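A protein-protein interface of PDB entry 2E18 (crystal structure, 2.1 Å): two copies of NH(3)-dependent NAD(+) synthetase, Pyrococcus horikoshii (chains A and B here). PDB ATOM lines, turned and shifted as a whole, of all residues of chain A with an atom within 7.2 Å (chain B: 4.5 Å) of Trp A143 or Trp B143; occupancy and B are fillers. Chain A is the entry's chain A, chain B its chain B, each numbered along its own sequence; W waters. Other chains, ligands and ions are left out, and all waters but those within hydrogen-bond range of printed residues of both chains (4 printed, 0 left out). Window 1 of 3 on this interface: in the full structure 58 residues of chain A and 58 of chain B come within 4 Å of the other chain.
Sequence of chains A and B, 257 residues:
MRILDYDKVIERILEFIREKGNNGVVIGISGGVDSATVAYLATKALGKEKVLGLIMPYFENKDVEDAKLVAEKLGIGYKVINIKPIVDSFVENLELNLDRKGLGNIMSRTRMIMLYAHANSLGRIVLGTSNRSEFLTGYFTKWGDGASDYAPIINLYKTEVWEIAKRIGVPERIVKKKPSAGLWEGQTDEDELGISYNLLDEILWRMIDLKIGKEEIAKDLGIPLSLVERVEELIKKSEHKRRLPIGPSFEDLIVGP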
ATOM      1  N   ASN A 105      -6.059  32.691   7.814  1.00  0.00           N
ATOM      2  CA  ASN A 105      -4.853  31.912   7.573  1.00  0.00           C
ATOM      3  C   ASN A 105      -3.753  32.774   6.956  1.00  0.00           C
ATOM      4  O   ASN A 105      -2.576  32.638   7.264  1.00  0.00           O
ATOM      5  CB  ASN A 105      -5.209  30.765   6.625  1.00  0.00           C
ATOM      6  CG  ASN A 105      -5.965  29.705   7.384  1.00  0.00           C
ATOM      7  OD1 ASN A 105      -6.518  28.770   6.814  1.00  0.00           O
ATOM      8  ND2 ASN A 105      -5.983  29.867   8.718  1.00  0.00           N
ATOM      9  N   SER A 108      -2.236  35.005   9.830  1.00  0.00           N
ATOM     10  CA  SER A 108      -1.383  34.217  10.718  1.00  0.00           C
ATOM     11  C   SER A 108      -0.058  33.828  10.043  1.00  0.00           C
ATOM     12  O   SER A 108       1.008  33.873  10.658  1.00  0.00           O
ATOM     13  CB  SER A 108      -2.144  32.960  11.175  1.00  0.00           C
ATOM     14  OG  SER A 108      -1.453  32.270  12.208  1.00  0.00           O
ATOM     15  N   ARG A 109      -0.130  33.440   8.779  1.00  0.00           N
ATOM     16  CA  ARG A 109       1.075  33.078   8.046  1.00  0.00           C
ATOM     17  C   ARG A 109       1.908  34.335   7.769  1.00  0.00           C
ATOM     18  O   ARG A 109       3.135  34.271   7.733  1.00  0.00           O
ATOM     19  CB  ARG A 109       0.691  32.364   6.744  1.00  0.00           C
ATOM     20  CG  ARG A 109       0.178  30.959   7.024  1.00  0.00           C
ATOM     21  CD  ARG A 109      -0.528  30.344   5.840  1.00  0.00           C
ATOM     22  NE  ARG A 109      -0.973  28.994   6.162  1.00  0.00           N
ATOM     23  CZ  ARG A 109      -2.041  28.411   5.626  1.00  0.00           C
ATOM     24  NH1 ARG A 109      -2.775  29.064   4.736  1.00  0.00           N
ATOM     25  NH2 ARG A 109      -2.381  27.182   5.993  1.00  0.00           N
ATOM     26  N   THR A 110       1.237  35.470   7.588  1.00  0.00           N
ATOM     27  CA  THR A 110       1.933  36.743   7.354  1.00  0.00           C
ATOM     28  C   THR A 110       2.690  37.116   8.636  1.00  0.00           C
ATOM     29  O   THR A 110       3.810  37.631   8.591  1.00  0.00           O
ATOM     30  CB  THR A 110       0.927  37.873   7.017  1.00  0.00           C
ATOM     31  OG1 THR A 110       0.324  37.602   5.748  1.00  0.00           O
ATOM     32  CG2 THR A 110       1.613  39.230   6.983  1.00  0.00           C
ATOM     33  N   MET A 112       3.834  35.001  10.745  1.00  0.00           N
ATOM     34  CA  MET A 112       4.947  34.057  10.827  1.00  0.00           C
ATOM     35  C   MET A 112       6.148  34.565  10.026  1.00  0.00           C
ATOM     36  O   MET A 112       7.285  34.508  10.494  1.00  0.00           O
ATOM     37  CB  MET A 112       4.517  32.672  10.317  1.00  0.00           C
ATOM     38  CG  MET A 112       5.628  31.623  10.315  1.00  0.00           C
ATOM     39  SD  MET A 112       6.557  31.514   8.757  1.00  0.00           S
ATOM     40  CE  MET A 112       8.055  32.201   9.126  1.00  0.00           C
ATOM     41  N   ILE A 113       5.902  35.060   8.815  1.00  0.00           N
ATOM     42  CA  ILE A 113       6.990  35.588   8.004  1.00  0.00           C
ATOM     43  C   ILE A 113       7.652  36.783   8.698  1.00  0.00           C
ATOM     44  O   ILE A 113       8.883  36.885   8.742  1.00  0.00           O
ATOM     45  CB  ILE A 113       6.489  35.980   6.595  1.00  0.00           C
ATOM     46  CG1 ILE A 113       6.030  34.719   5.848  1.00  0.00           C
ATOM     47  CG2 ILE A 113       7.596  36.667   5.819  1.00  0.00           C
ATOM     48  CD1 ILE A 113       5.566  34.962   4.422  1.00  0.00           C
ATOM     49  N   TYR A 116       9.844  35.507  11.710  1.00  0.00           N
ATOM     50  CA  TYR A 116      11.090  34.929  11.239  1.00  0.00           C
ATOM     51  C   TYR A 116      12.013  35.931  10.559  1.00  0.00           C
ATOM     52  O   TYR A 116      13.230  35.809  10.667  1.00  0.00           O
ATOM     53  CB  TYR A 116      10.830  33.739  10.310  1.00  0.00           C
ATOM     54  CG  TYR A 116      10.680  32.438  11.067  1.00  0.00           C
ATOM     55  CD1 TYR A 116       9.455  32.061  11.617  1.00  0.00           C
ATOM     56  CD2 TYR A 116      11.782  31.606  11.285  1.00  0.00           C
ATOM     57  CE1 TYR A 116       9.325  30.890  12.367  1.00  0.00           C
ATOM     58  CE2 TYR A 116      11.662  30.427  12.037  1.00  0.00           C
ATOM     59  CZ  TYR A 116      10.432  30.079  12.575  1.00  0.00           C
ATOM     60  OH  TYR A 116      10.308  28.934  13.338  1.00  0.00           O
ATOM     61  N   VAL A 126      12.480  32.126  17.156  1.00  0.00           N
ATOM     62  CA  VAL A 126      11.082  32.522  17.301  1.00  0.00           C
ATOM     63  C   VAL A 126      10.423  31.599  18.315  1.00  0.00           C
ATOM     64  O   VAL A 126      10.514  30.383  18.196  1.00  0.00           O
ATOM     65  CB  VAL A 126      10.297  32.401  15.977  1.00  0.00           C
ATOM     66  CG1 VAL A 126       8.820  32.712  16.221  1.00  0.00           C
ATOM     67  CG2 VAL A 126      10.867  33.351  14.939  1.00  0.00           C
ATOM     68  N   PHE A 140      -5.555  25.993  15.015  1.00  0.00           N
ATOM     69  CA  PHE A 140      -4.429  26.853  14.694  1.00  0.00           C
ATOM     70  C   PHE A 140      -4.196  26.785  13.198  1.00  0.00           C
ATOM     71  O   PHE A 140      -4.640  25.844  12.542  1.00  0.00           O
ATOM     72  CB  PHE A 140      -3.171  26.415  15.460  1.00  0.00           C
ATOM     73  CG  PHE A 140      -2.723  25.012  15.162  1.00  0.00           C
ATOM     74  CD1 PHE A 140      -1.866  24.752  14.098  1.00  0.00           C
ATOM     75  CD2 PHE A 140      -3.143  23.949  15.965  1.00  0.00           C
ATOM     76  CE1 PHE A 140      -1.423  23.447  13.830  1.00  0.00           C
ATOM     77  CE2 PHE A 140      -2.712  22.645  15.710  1.00  0.00           C
ATOM     78  CZ  PHE A 140      -1.846  22.394  14.638  1.00  0.00           C
ATOM     79  N   THR A 141      -3.520  27.793  12.662  1.00  0.00           N
ATOM     80  CA  THR A 141      -3.235  27.840  11.237  1.00  0.00           C
ATOM     81  C   THR A 141      -1.980  27.050  10.940  1.00  0.00           C
ATOM     82  O   THR A 141      -0.925  27.280  11.541  1.00  0.00           O
ATOM     83  CB  THR A 141      -3.015  29.281  10.746  1.00  0.00           C
ATOM     84  OG1 THR A 141      -4.193  30.054  10.997  1.00  0.00           O
ATOM     85  CG2 THR A 141      -2.699  29.293   9.248  1.00  0.00           C
ATOM     86  N   LYS A 142      -2.093  26.115  10.012  1.00  0.00           N
ATOM     87  CA  LYS A 142      -0.951  25.303   9.627  1.00  0.00           C
ATOM     88  C   LYS A 142       0.073  26.216   8.969  1.00  0.00           C
ATOM     89  O   LYS A 142      -0.268  26.979   8.066  1.00  0.00           O
ATOM     90  CB  LYS A 142      -1.401  24.203   8.658  1.00  0.00           C
ATOM     91  CG  LYS A 142      -0.307  23.227   8.277  1.00  0.00           C
ATOM     92  CD  LYS A 142      -0.892  21.909   7.774  1.00  0.00           C
ATOM     93  CE  LYS A 142      -1.725  22.082   6.517  1.00  0.00           C
ATOM     94  NZ  LYS A 142      -2.349  20.789   6.119  1.00  0.00           N
ATOM     95  N   TRP A 143       1.318  26.153   9.437  1.00  0.00           N
ATOM     96  CA  TRP A 143       2.406  26.973   8.894  1.00  0.00           C
ATOM     97  C   TRP A 143       2.251  28.467   9.219  1.00  0.00           C
ATOM     98  O   TRP A 143       3.004  29.290   8.705  1.00  0.00           O
ATOM     99  CB  TRP A 143       2.487  26.834   7.366  1.00  0.00           C
ATOM    100  CG  TRP A 143       2.337  25.444   6.828  1.00  0.00           C
ATOM    101  CD1 TRP A 143       1.665  25.081   5.696  1.00  0.00           C
ATOM    102  CD2 TRP A 143       2.901  24.241   7.359  1.00  0.00           C
ATOM    103  NE1 TRP A 143       1.773  23.734   5.489  1.00  0.00           N
ATOM    104  CE2 TRP A 143       2.526  23.189   6.494  1.00  0.00           C
ATOM    105  CE3 TRP A 143       3.687  23.947   8.480  1.00  0.00           C
ATOM    106  CZ2 TRP A 143       2.909  21.860   6.717  1.00  0.00           C
ATOM    107  CZ3 TRP A 143       4.070  22.628   8.702  1.00  0.00           C
ATOM    108  CH2 TRP A 143       3.679  21.599   7.825  1.00  0.00           C
ATOM    109  N   GLY A 144       1.271  28.819  10.049  1.00  0.00           N
ATOM    110  CA  GLY A 144       1.074  30.219  10.391  1.00  0.00           C
ATOM    111  C   GLY A 144       1.553  30.494  11.800  1.00  0.00           C
ATOM    112  O   GLY A 144       2.684  30.151  12.151  1.00  0.00           O
ATOM    113  N   ASP A 145       0.708  31.134  12.601  1.00  0.00           N
ATOM    114  CA  ASP A 145       1.055  31.385  13.988  1.00  0.00           C
ATOM    115  C   ASP A 145       1.175  29.963  14.520  1.00  0.00           C
ATOM    116  O   ASP A 145       0.465  29.055  14.059  1.00  0.00           O
ATOM    117  CB  ASP A 145      -0.062  32.142  14.739  1.00  0.00           C
ATOM    118  CG  ASP A 145      -0.121  33.628  14.382  1.00  0.00           C
ATOM    119  OD1 ASP A 145       0.940  34.287  14.395  1.00  0.00           O
ATOM    120  OD2 ASP A 145      -1.232  34.144  14.104  1.00  0.00           O
ATOM    121  N   GLY A 146       2.074  29.763  15.471  1.00  0.00           N
ATOM    122  CA  GLY A 146       2.282  28.437  16.008  1.00  0.00           C
ATOM    123  C   GLY A 146       3.598  27.933  15.456  1.00  0.00           C
ATOM    124  O   GLY A 146       4.448  27.463  16.210  1.00  0.00           O
ATOM    125  N   ALA A 147       3.764  28.035  14.136  1.00  0.00           N
ATOM    126  CA  ALA A 147       4.992  27.593  13.486  1.00  0.00           C
ATOM    127  C   ALA A 147       6.128  28.437  14.052  1.00  0.00           C
ATOM    128  O   ALA A 147       6.162  29.654  13.881  1.00  0.00           O
ATOM    129  CB  ALA A 147       4.889  27.774  11.979  1.00  0.00           C
ATOM    130  N   SER A 148       7.051  27.785  14.744  1.00  0.00           N
ATOM    131  CA  SER A 148       8.158  28.490  15.363  1.00  0.00           C
ATOM    132  C   SER A 148       9.341  27.555  15.548  1.00  0.00           C
ATOM    133  O   SER A 148       9.336  26.441  15.032  1.00  0.00           O
ATOM    134  CB  SER A 148       7.711  29.024  16.716  1.00  0.00           C
ATOM    135  OG  SER A 148       7.154  27.968  17.480  1.00  0.00           O
ATOM    136  N   ASP A 149      10.351  28.018  16.281  1.00  0.00           N
ATOM    137  CA  ASP A 149      11.535  27.216  16.529  1.00  0.00           C
ATOM    138  C   ASP A 149      11.318  26.398  17.789  1.00  0.00           C
ATOM    139  O   ASP A 149      11.681  25.224  17.852  1.00  0.00           O
ATOM    140  CB  ASP A 149      12.763  28.122  16.648  1.00  0.00           C
ATOM    141  CG  ASP A 149      13.020  28.893  15.368  1.00  0.00           C
ATOM    142  OD1 ASP A 149      13.047  28.237  14.300  1.00  0.00           O
ATOM    143  OD2 ASP A 149      13.182  30.137  15.419  1.00  0.00           O
ATOM    144  N   HIS A 240      -3.748  15.832  10.463  1.00  0.00           N
ATOM    145  CA  HIS A 240      -2.884  16.293   9.382  1.00  0.00           C
ATOM    146  C   HIS A 240      -2.126  17.564   9.754  1.00  0.00           C
ATOM    147  O   HIS A 240      -1.176  17.939   9.075  1.00  0.00           O
ATOM    148  CB  HIS A 240      -3.702  16.509   8.096  1.00  0.00           C
ATOM    149  CG  HIS A 240      -4.644  17.671   8.153  1.00  0.00           C
ATOM    150  ND1 HIS A 240      -4.296  18.937   7.729  1.00  0.00           N
ATOM    151  CD2 HIS A 240      -5.924  17.761   8.588  1.00  0.00           C
ATOM    152  CE1 HIS A 240      -5.319  19.755   7.900  1.00  0.00           C
ATOM    153  NE2 HIS A 240      -6.320  19.068   8.422  1.00  0.00           N
ATOM    154  N   LYS A 241      -2.542  18.220  10.838  1.00  0.00           N
ATOM    155  CA  LYS A 241      -1.874  19.435  11.297  1.00  0.00           C
ATOM    156  C   LYS A 241      -0.781  19.147  12.322  1.00  0.00           C
ATOM    157  O   LYS A 241      -0.060  20.053  12.725  1.00  0.00           O
ATOM    158  CB  LYS A 241      -2.869  20.408  11.929  1.00  0.00           C
ATOM    159  CG  LYS A 241      -3.860  21.026  10.967  1.00  0.00           C
ATOM    160  CD  LYS A 241      -4.616  22.132  11.662  1.00  0.00           C
ATOM    161  CE  LYS A 241      -5.625  22.776  10.749  1.00  0.00           C
ATOM    162  NZ  LYS A 241      -6.247  23.940  11.423  1.00  0.00           N
ATOM    163  N   ARG A 243       1.794  16.860  11.927  1.00  0.00           N
ATOM    164  CA  ARG A 243       2.841  16.085  11.282  1.00  0.00           C
ATOM    165  C   ARG A 243       3.353  16.842  10.063  1.00  0.00           C
ATOM    166  O   ARG A 243       2.618  17.622   9.455  1.00  0.00           O
ATOM    167  CB  ARG A 243       2.298  14.719  10.858  1.00  0.00           C
ATOM    168  CG  ARG A 243       1.157  14.793   9.857  1.00  0.00           C
ATOM    169  CD  ARG A 243       0.604  13.410   9.577  1.00  0.00           C
ATOM    170  NE  ARG A 243       0.063  12.800  10.790  1.00  0.00           N
ATOM    171  CZ  ARG A 243      -0.425  11.567  10.854  1.00  0.00           C
ATOM    172  NH1 ARG A 243      -0.444  10.799   9.770  1.00  0.00           N
ATOM    173  NH2 ARG A 243      -0.898  11.101  12.001  1.00  0.00           N
ATOM    174  N   LEU A 244       4.619  16.630   9.721  1.00  0.00           N
ATOM    175  CA  LEU A 244       5.195  17.287   8.557  1.00  0.00           C
ATOM    176  C   LEU A 244       4.632  16.596   7.314  1.00  0.00           C
ATOM    177  O   LEU A 244       4.145  15.471   7.395  1.00  0.00           O
ATOM    178  CB  LEU A 244       6.724  17.181   8.589  1.00  0.00           C
ATOM    179  CG  LEU A 244       7.421  17.874   9.767  1.00  0.00           C
ATOM    180  CD1 LEU A 244       8.921  17.693   9.643  1.00  0.00           C
ATOM    181  CD2 LEU A 244       7.072  19.361   9.792  1.00  0.00           C
ATOM    182  N   PRO A 245       4.691  17.261   6.148  1.00  0.00           N
ATOM    183  CA  PRO A 245       4.175  16.689   4.897  1.00  0.00           C
ATOM    184  C   PRO A 245       4.672  15.273   4.629  1.00  0.00           C
ATOM    185  O   PRO A 245       5.871  15.017   4.638  1.00  0.00           O
ATOM    186  CB  PRO A 245       4.669  17.671   3.842  1.00  0.00           C
ATOM    187  CG  PRO A 245       4.681  18.973   4.582  1.00  0.00           C
ATOM    188  CD  PRO A 245       5.306  18.577   5.900  1.00  0.00           C
ATOM    189  N   ARG B 109       8.425  31.512   1.797  1.00  0.00           N
ATOM    190  CA  ARG B 109       7.240  31.550   2.639  1.00  0.00           C
ATOM    191  C   ARG B 109       6.096  32.297   1.957  1.00  0.00           C
ATOM    192  O   ARG B 109       4.937  31.904   2.082  1.00  0.00           O
ATOM    193  CB  ARG B 109       7.594  32.162   4.001  1.00  0.00           C
ATOM    194  CG  ARG B 109       8.504  31.232   4.783  1.00  0.00           C
ATOM    195  CD  ARG B 109       9.159  31.864   5.995  1.00  0.00           C
ATOM    196  NE  ARG B 109       9.965  30.859   6.677  1.00  0.00           N
ATOM    197  CZ  ARG B 109      11.112  31.095   7.306  1.00  0.00           C
ATOM    198  NH1 ARG B 109      11.616  32.320   7.358  1.00  0.00           N
ATOM    199  NH2 ARG B 109      11.760  30.088   7.877  1.00  0.00           N
ATOM    200  N   MET B 112       4.429  30.017  -0.257  1.00  0.00           N
ATOM    201  CA  MET B 112       3.605  29.081   0.510  1.00  0.00           C
ATOM    202  C   MET B 112       2.231  29.693   0.755  1.00  0.00           C
ATOM    203  O   MET B 112       1.211  29.035   0.555  1.00  0.00           O
ATOM    204  CB  MET B 112       4.284  28.731   1.849  1.00  0.00           C
ATOM    205  CG  MET B 112       3.462  27.809   2.767  1.00  0.00           C
ATOM    206  SD  MET B 112       2.439  28.695   3.978  1.00  0.00           S
ATOM    207  CE  MET B 112       0.875  28.743   3.279  1.00  0.00           C
ATOM    208  N   TYR B 116      -1.428  28.213  -0.625  1.00  0.00           N
ATOM    209  CA  TYR B 116      -2.547  27.877   0.256  1.00  0.00           C
ATOM    210  C   TYR B 116      -3.761  28.782   0.069  1.00  0.00           C
ATOM    211  O   TYR B 116      -4.893  28.357   0.299  1.00  0.00           O
ATOM    212  CB  TYR B 116      -2.114  27.904   1.729  1.00  0.00           C
ATOM    213  CG  TYR B 116      -1.520  26.593   2.196  1.00  0.00           C
ATOM    214  CD1 TYR B 116      -0.174  26.292   1.985  1.00  0.00           C
ATOM    215  CD2 TYR B 116      -2.323  25.631   2.802  1.00  0.00           C
ATOM    216  CE1 TYR B 116       0.359  25.056   2.364  1.00  0.00           C
ATOM    217  CE2 TYR B 116      -1.809  24.402   3.181  1.00  0.00           C
ATOM    218  CZ  TYR B 116      -0.471  24.115   2.959  1.00  0.00           C
ATOM    219  OH  TYR B 116       0.016  22.876   3.302  1.00  0.00           O
ATOM    220  N   THR B 141      13.434  25.847   2.947  1.00  0.00           N
ATOM    221  CA  THR B 141      13.010  26.874   3.881  1.00  0.00           C
ATOM    222  C   THR B 141      11.998  26.318   4.877  1.00  0.00           C
ATOM    223  O   THR B 141      10.986  25.746   4.487  1.00  0.00           O
ATOM    224  CB  THR B 141      12.358  28.068   3.152  1.00  0.00           C
ATOM    225  OG1 THR B 141      13.303  28.659   2.251  1.00  0.00           O
ATOM    226  CG2 THR B 141      11.888  29.121   4.170  1.00  0.00           C
ATOM    227  N   LYS B 142      12.276  26.491   6.161  1.00  0.00           N
ATOM    228  CA  LYS B 142      11.359  26.024   7.184  1.00  0.00           C
ATOM    229  C   LYS B 142      10.049  26.796   7.000  1.00  0.00           C
ATOM    230  O   LYS B 142      10.060  28.016   6.873  1.00  0.00           O
ATOM    231  CB  LYS B 142      11.932  26.290   8.584  1.00  0.00           C
ATOM    232  CG  LYS B 142      11.046  25.796   9.714  1.00  0.00           C
ATOM    233  CD  LYS B 142      11.537  26.249  11.093  1.00  0.00           C
ATOM    234  CE  LYS B 142      12.886  25.654  11.448  1.00  0.00           C
ATOM    235  NZ  LYS B 142      13.227  25.899  12.878  1.00  0.00           N
ATOM    236  N   TRP B 143       8.933  26.076   6.958  1.00  0.00           N
ATOM    237  CA  TRP B 143       7.613  26.678   6.792  1.00  0.00           C
ATOM    238  C   TRP B 143       7.460  27.314   5.406  1.00  0.00           C
ATOM    239  O   TRP B 143       6.466  27.982   5.135  1.00  0.00           O
ATOM    240  CB  TRP B 143       7.366  27.752   7.868  1.00  0.00           C
ATOM    241  CG  TRP B 143       7.778  27.380   9.281  1.00  0.00           C
ATOM    242  CD1 TRP B 143       8.344  28.216  10.205  1.00  0.00           C
ATOM    243  CD2 TRP B 143       7.654  26.101   9.928  1.00  0.00           C
ATOM    244  NE1 TRP B 143       8.584  27.542  11.374  1.00  0.00           N
ATOM    245  CE2 TRP B 143       8.171  26.243  11.236  1.00  0.00           C
ATOM    246  CE3 TRP B 143       7.160  24.851   9.529  1.00  0.00           C
ATOM    247  CZ2 TRP B 143       8.212  25.180  12.151  1.00  0.00           C
ATOM    248  CZ3 TRP B 143       7.199  23.789  10.440  1.00  0.00           C
ATOM    249  CH2 TRP B 143       7.723  23.962  11.736  1.00  0.00           C
ATOM    250  N   GLY B 144       8.446  27.111   4.533  1.00  0.00           N
ATOM    251  CA  GLY B 144       8.375  27.660   3.184  1.00  0.00           C
ATOM    252  C   GLY B 144       7.869  26.621   2.180  1.00  0.00           C
ATOM    253  O   GLY B 144       6.778  26.080   2.296  1.00  0.00           O
ATOM    254  N   ALA B 147       6.587  23.292   3.113  1.00  0.00           N
ATOM    255  CA  ALA B 147       5.279  23.205   3.754  1.00  0.00           C
ATOM    256  C   ALA B 147       4.157  23.000   2.732  1.00  0.00           C
ATOM    257  O   ALA B 147       3.948  23.804   1.833  1.00  0.00           O
ATOM    258  CB  ALA B 147       5.039  24.495   4.539  1.00  0.00           C
ATOM    259  N   SER B 148       3.442  21.892   2.867  1.00  0.00           N
ATOM    260  CA  SER B 148       2.369  21.544   1.949  1.00  0.00           C
ATOM    261  C   SER B 148       1.515  20.487   2.627  1.00  0.00           C
ATOM    262  O   SER B 148       1.793  20.093   3.760  1.00  0.00           O
ATOM    263  CB  SER B 148       2.944  20.957   0.670  1.00  0.00           C
ATOM    264  OG  SER B 148       3.608  19.740   0.961  1.00  0.00           O
ATOM    265  N   ARG B 243      11.047  18.478  12.318  1.00  0.00           N
ATOM    266  CA  ARG B 243      10.115  18.257  13.421  1.00  0.00           C
ATOM    267  C   ARG B 243       9.217  19.466  13.662  1.00  0.00           C
ATOM    268  O   ARG B 243       9.529  20.585  13.243  1.00  0.00           O
ATOM    269  CB  ARG B 243      10.878  17.940  14.713  1.00  0.00           C
ATOM    270  CG  ARG B 243      11.749  19.086  15.213  1.00  0.00           C
ATOM    271  CD  ARG B 243      12.139  18.908  16.675  1.00  0.00           C
ATOM    272  NE  ARG B 243      12.822  20.086  17.205  1.00  0.00           N
ATOM    273  CZ  ARG B 243      14.139  20.272  17.186  1.00  0.00           C
ATOM    274  NH1 ARG B 243      14.940  19.352  16.665  1.00  0.00           N
ATOM    275  NH2 ARG B 243      14.657  21.388  17.687  1.00  0.00           N
ATOM    276  N   LEU B 244       8.092  19.243  14.333  1.00  0.00           N
ATOM    277  CA  LEU B 244       7.195  20.347  14.646  1.00  0.00           C
ATOM    278  C   LEU B 244       7.723  21.025  15.907  1.00  0.00           C
ATOM    279  O   LEU B 244       8.465  20.416  16.686  1.00  0.00           O
ATOM    280  CB  LEU B 244       5.760  19.849  14.864  1.00  0.00           C
ATOM    281  CG  LEU B 244       5.023  19.414  13.589  1.00  0.00           C
ATOM    282  CD1 LEU B 244       3.539  19.243  13.880  1.00  0.00           C
ATOM    283  CD2 LEU B 244       5.213  20.466  12.503  1.00  0.00           C
ATOM    284  N   PRO B 245       7.366  22.300  16.119  1.00  0.00           N
ATOM    285  CA  PRO B 245       7.822  23.047  17.297  1.00  0.00           C
ATOM    286  C   PRO B 245       7.655  22.255  18.594  1.00  0.00           C
ATOM    287  O   PRO B 245       6.557  21.813  18.913  1.00  0.00           O
ATOM    288  CB  PRO B 245       6.942  24.292  17.267  1.00  0.00           C
ATOM    289  CG  PRO B 245       6.737  24.511  15.800  1.00  0.00           C
ATOM    290  CD  PRO B 245       6.430  23.112  15.321  1.00  0.00           C
HETATM  291  O   HOH W   1       0.994  18.573   6.487  1.00  0.00           O
HETATM  292  O   HOH W   2      11.235  22.544  17.670  1.00  0.00           O
HETATM  293  O   HOH W   3      14.278  24.538  16.515  1.00  0.00           O
HETATM  294  O   HOH W   4      10.552  35.017   6.918  1.00  0.00           O
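The guanidinium group (NE) of Arg A109 sits at hydrogen-bond distance from the backbone carbonyl oxygen (O) of Lys A142, at 2.9 Å. The side-chain hydroxyl (OH) of Tyr A116 lies close to the backbone carbonyl oxygen (O) of Ser A148 (3.2 Å). OH of Tyr A116 lies within hydrogen-bond range of OD1 of Asp A149 (3.0 Å). The side-chain carboxylate of Asp A149 lies within hydrogen-bond range of the backbone NH of Val A126 (2.7 Å). A ring nitrogen (ND1) of His A240 sits at hydrogen-bond distance from the side-chain amino group (NZ) of Lys A142 (3.1 Å). The backbone carbonyl oxygen of Lys B142 sits at hydrogen-bond distance from the guanidinium group of Arg B109, at 2.9 Å.
Among the printed residues, pairs that only touch across the chains: Arg A109 with Met B112 (3.3 Å), Arg A109 with Tyr B116 (3.3 Å), Met A112 with Arg B109 (3.3 Å), Met A112 with Trp B143 (3.9 Å), Ile A113 with Arg B109 (3.5 Å), Tyr A116 with Arg B109 (3.4 Å), Tyr A116 with Lys B142 (3.7 Å), Lys A142 with Tyr B116 (3.7 Å), Trp A143 with Met B112 (3.9 Å), Trp A143 with Trp B143 (3.7 Å), Trp A143 with Ala B147 (3.4 Å), Trp A143 with Ser B148 (3.6 Å), Gly A146 with Pro B245 (3.8 Å), Ala A147 with Trp B143 (3.7 Å), Ser A148 with Trp B143 (3.3 Å), Ser A148 with Pro B245 (3.3 Å), Lys A241 with Leu B244 (3.9 Å), Arg A243 with Leu B244 (3.5 Å), Leu A244 with Arg B243 (3.5 Å), Leu A244 with Leu B244 (3.5 Å) and Pro A245 with Ser B148 (3.2 Å).
Tyr A116 touches Lys B142, and with the chains exchanged Lys A142 touches Tyr B116. Tyr A116 touches Trp B143, and with the chains exchanged Trp A143 touches Tyr B116. Arg A243 touches Leu B244, and with the chains exchanged Leu A244 touches Arg B243. Leu A244 touches its own counterpart, Leu B244. Positions printed for both chains: 109, 112, 116, 141, 142, 143, 144, 147, 148, 243, 244 and 245.
Ser A108 touches none of the printed residues of chain B. Of the printed residues of chain B, Tyr A116 touches Arg B109, Lys B142 and Trp B143. Trp A143 touches five residues of chain B. Printed residues of chain A within 4 Å of Arg B109: Met A112, Ile A113 and Tyr A116. Printed residues of chain A within 4 Å of Met B112: Arg A109 and Trp A143. Trp B143 touches just these residues of chain A: Met A112 (3.9 Å), Tyr A116 (3.0 Å), Trp A143 (3.7 Å), Ala A147 (3.7 Å) and Ser A148 (3.3 Å). The nearest residue of chain A that does not touch Trp B143 is Leu A244 (4.5 Å). The nearest printed residue of chain A that does not touch Ser B148 is Lys A142 (4.8 Å).
Hydrophobic or aromatic side chains of chain A within 4 Å of the printed part of chain B: Met A112, Ile A113, Tyr A116, Trp A143, Ala A147, Leu A244 and Pro A245. Among the printed residues, Asp or Glu carboxylates within 4 Å of a Lys or Arg side-chain nitrogen of the other chain: Asp A149 with Lys B142 (2.7 Å).
The side-chain hydroxyl of Tyr A116 sits at hydrogen-bond distance from the indole nitrogen of Trp B143, 3.0 Å away. The indole nitrogen of Trp A143 lies within hydrogen-bond range of the side-chain hydroxyl of Tyr B116 (2.9 Å). The side-chain carboxylate (OD1) of Asp A149 lies within salt-bridge range of the side-chain amino group (NZ) of Lys B142, at 2.7 Å.
Water W2 lies within hydrogen-bond range of O of Asp A149 and NE of Arg B243. Water W4 bridges the guanidinium group of Arg B109 and the backbone carbonyl oxygen of Ile A113. Water W3 bridges the backbone carbonyl oxygen of Asp A149 (3.0 Å) and the guanidinium group of Arg B243 (3.4 Å). Water W1 lies within hydrogen-bond range of the backbone carbonyl oxygen of Ser B148 (3.2 Å) and the backbone carbonyl oxygen of His A240 (3.4 Å).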
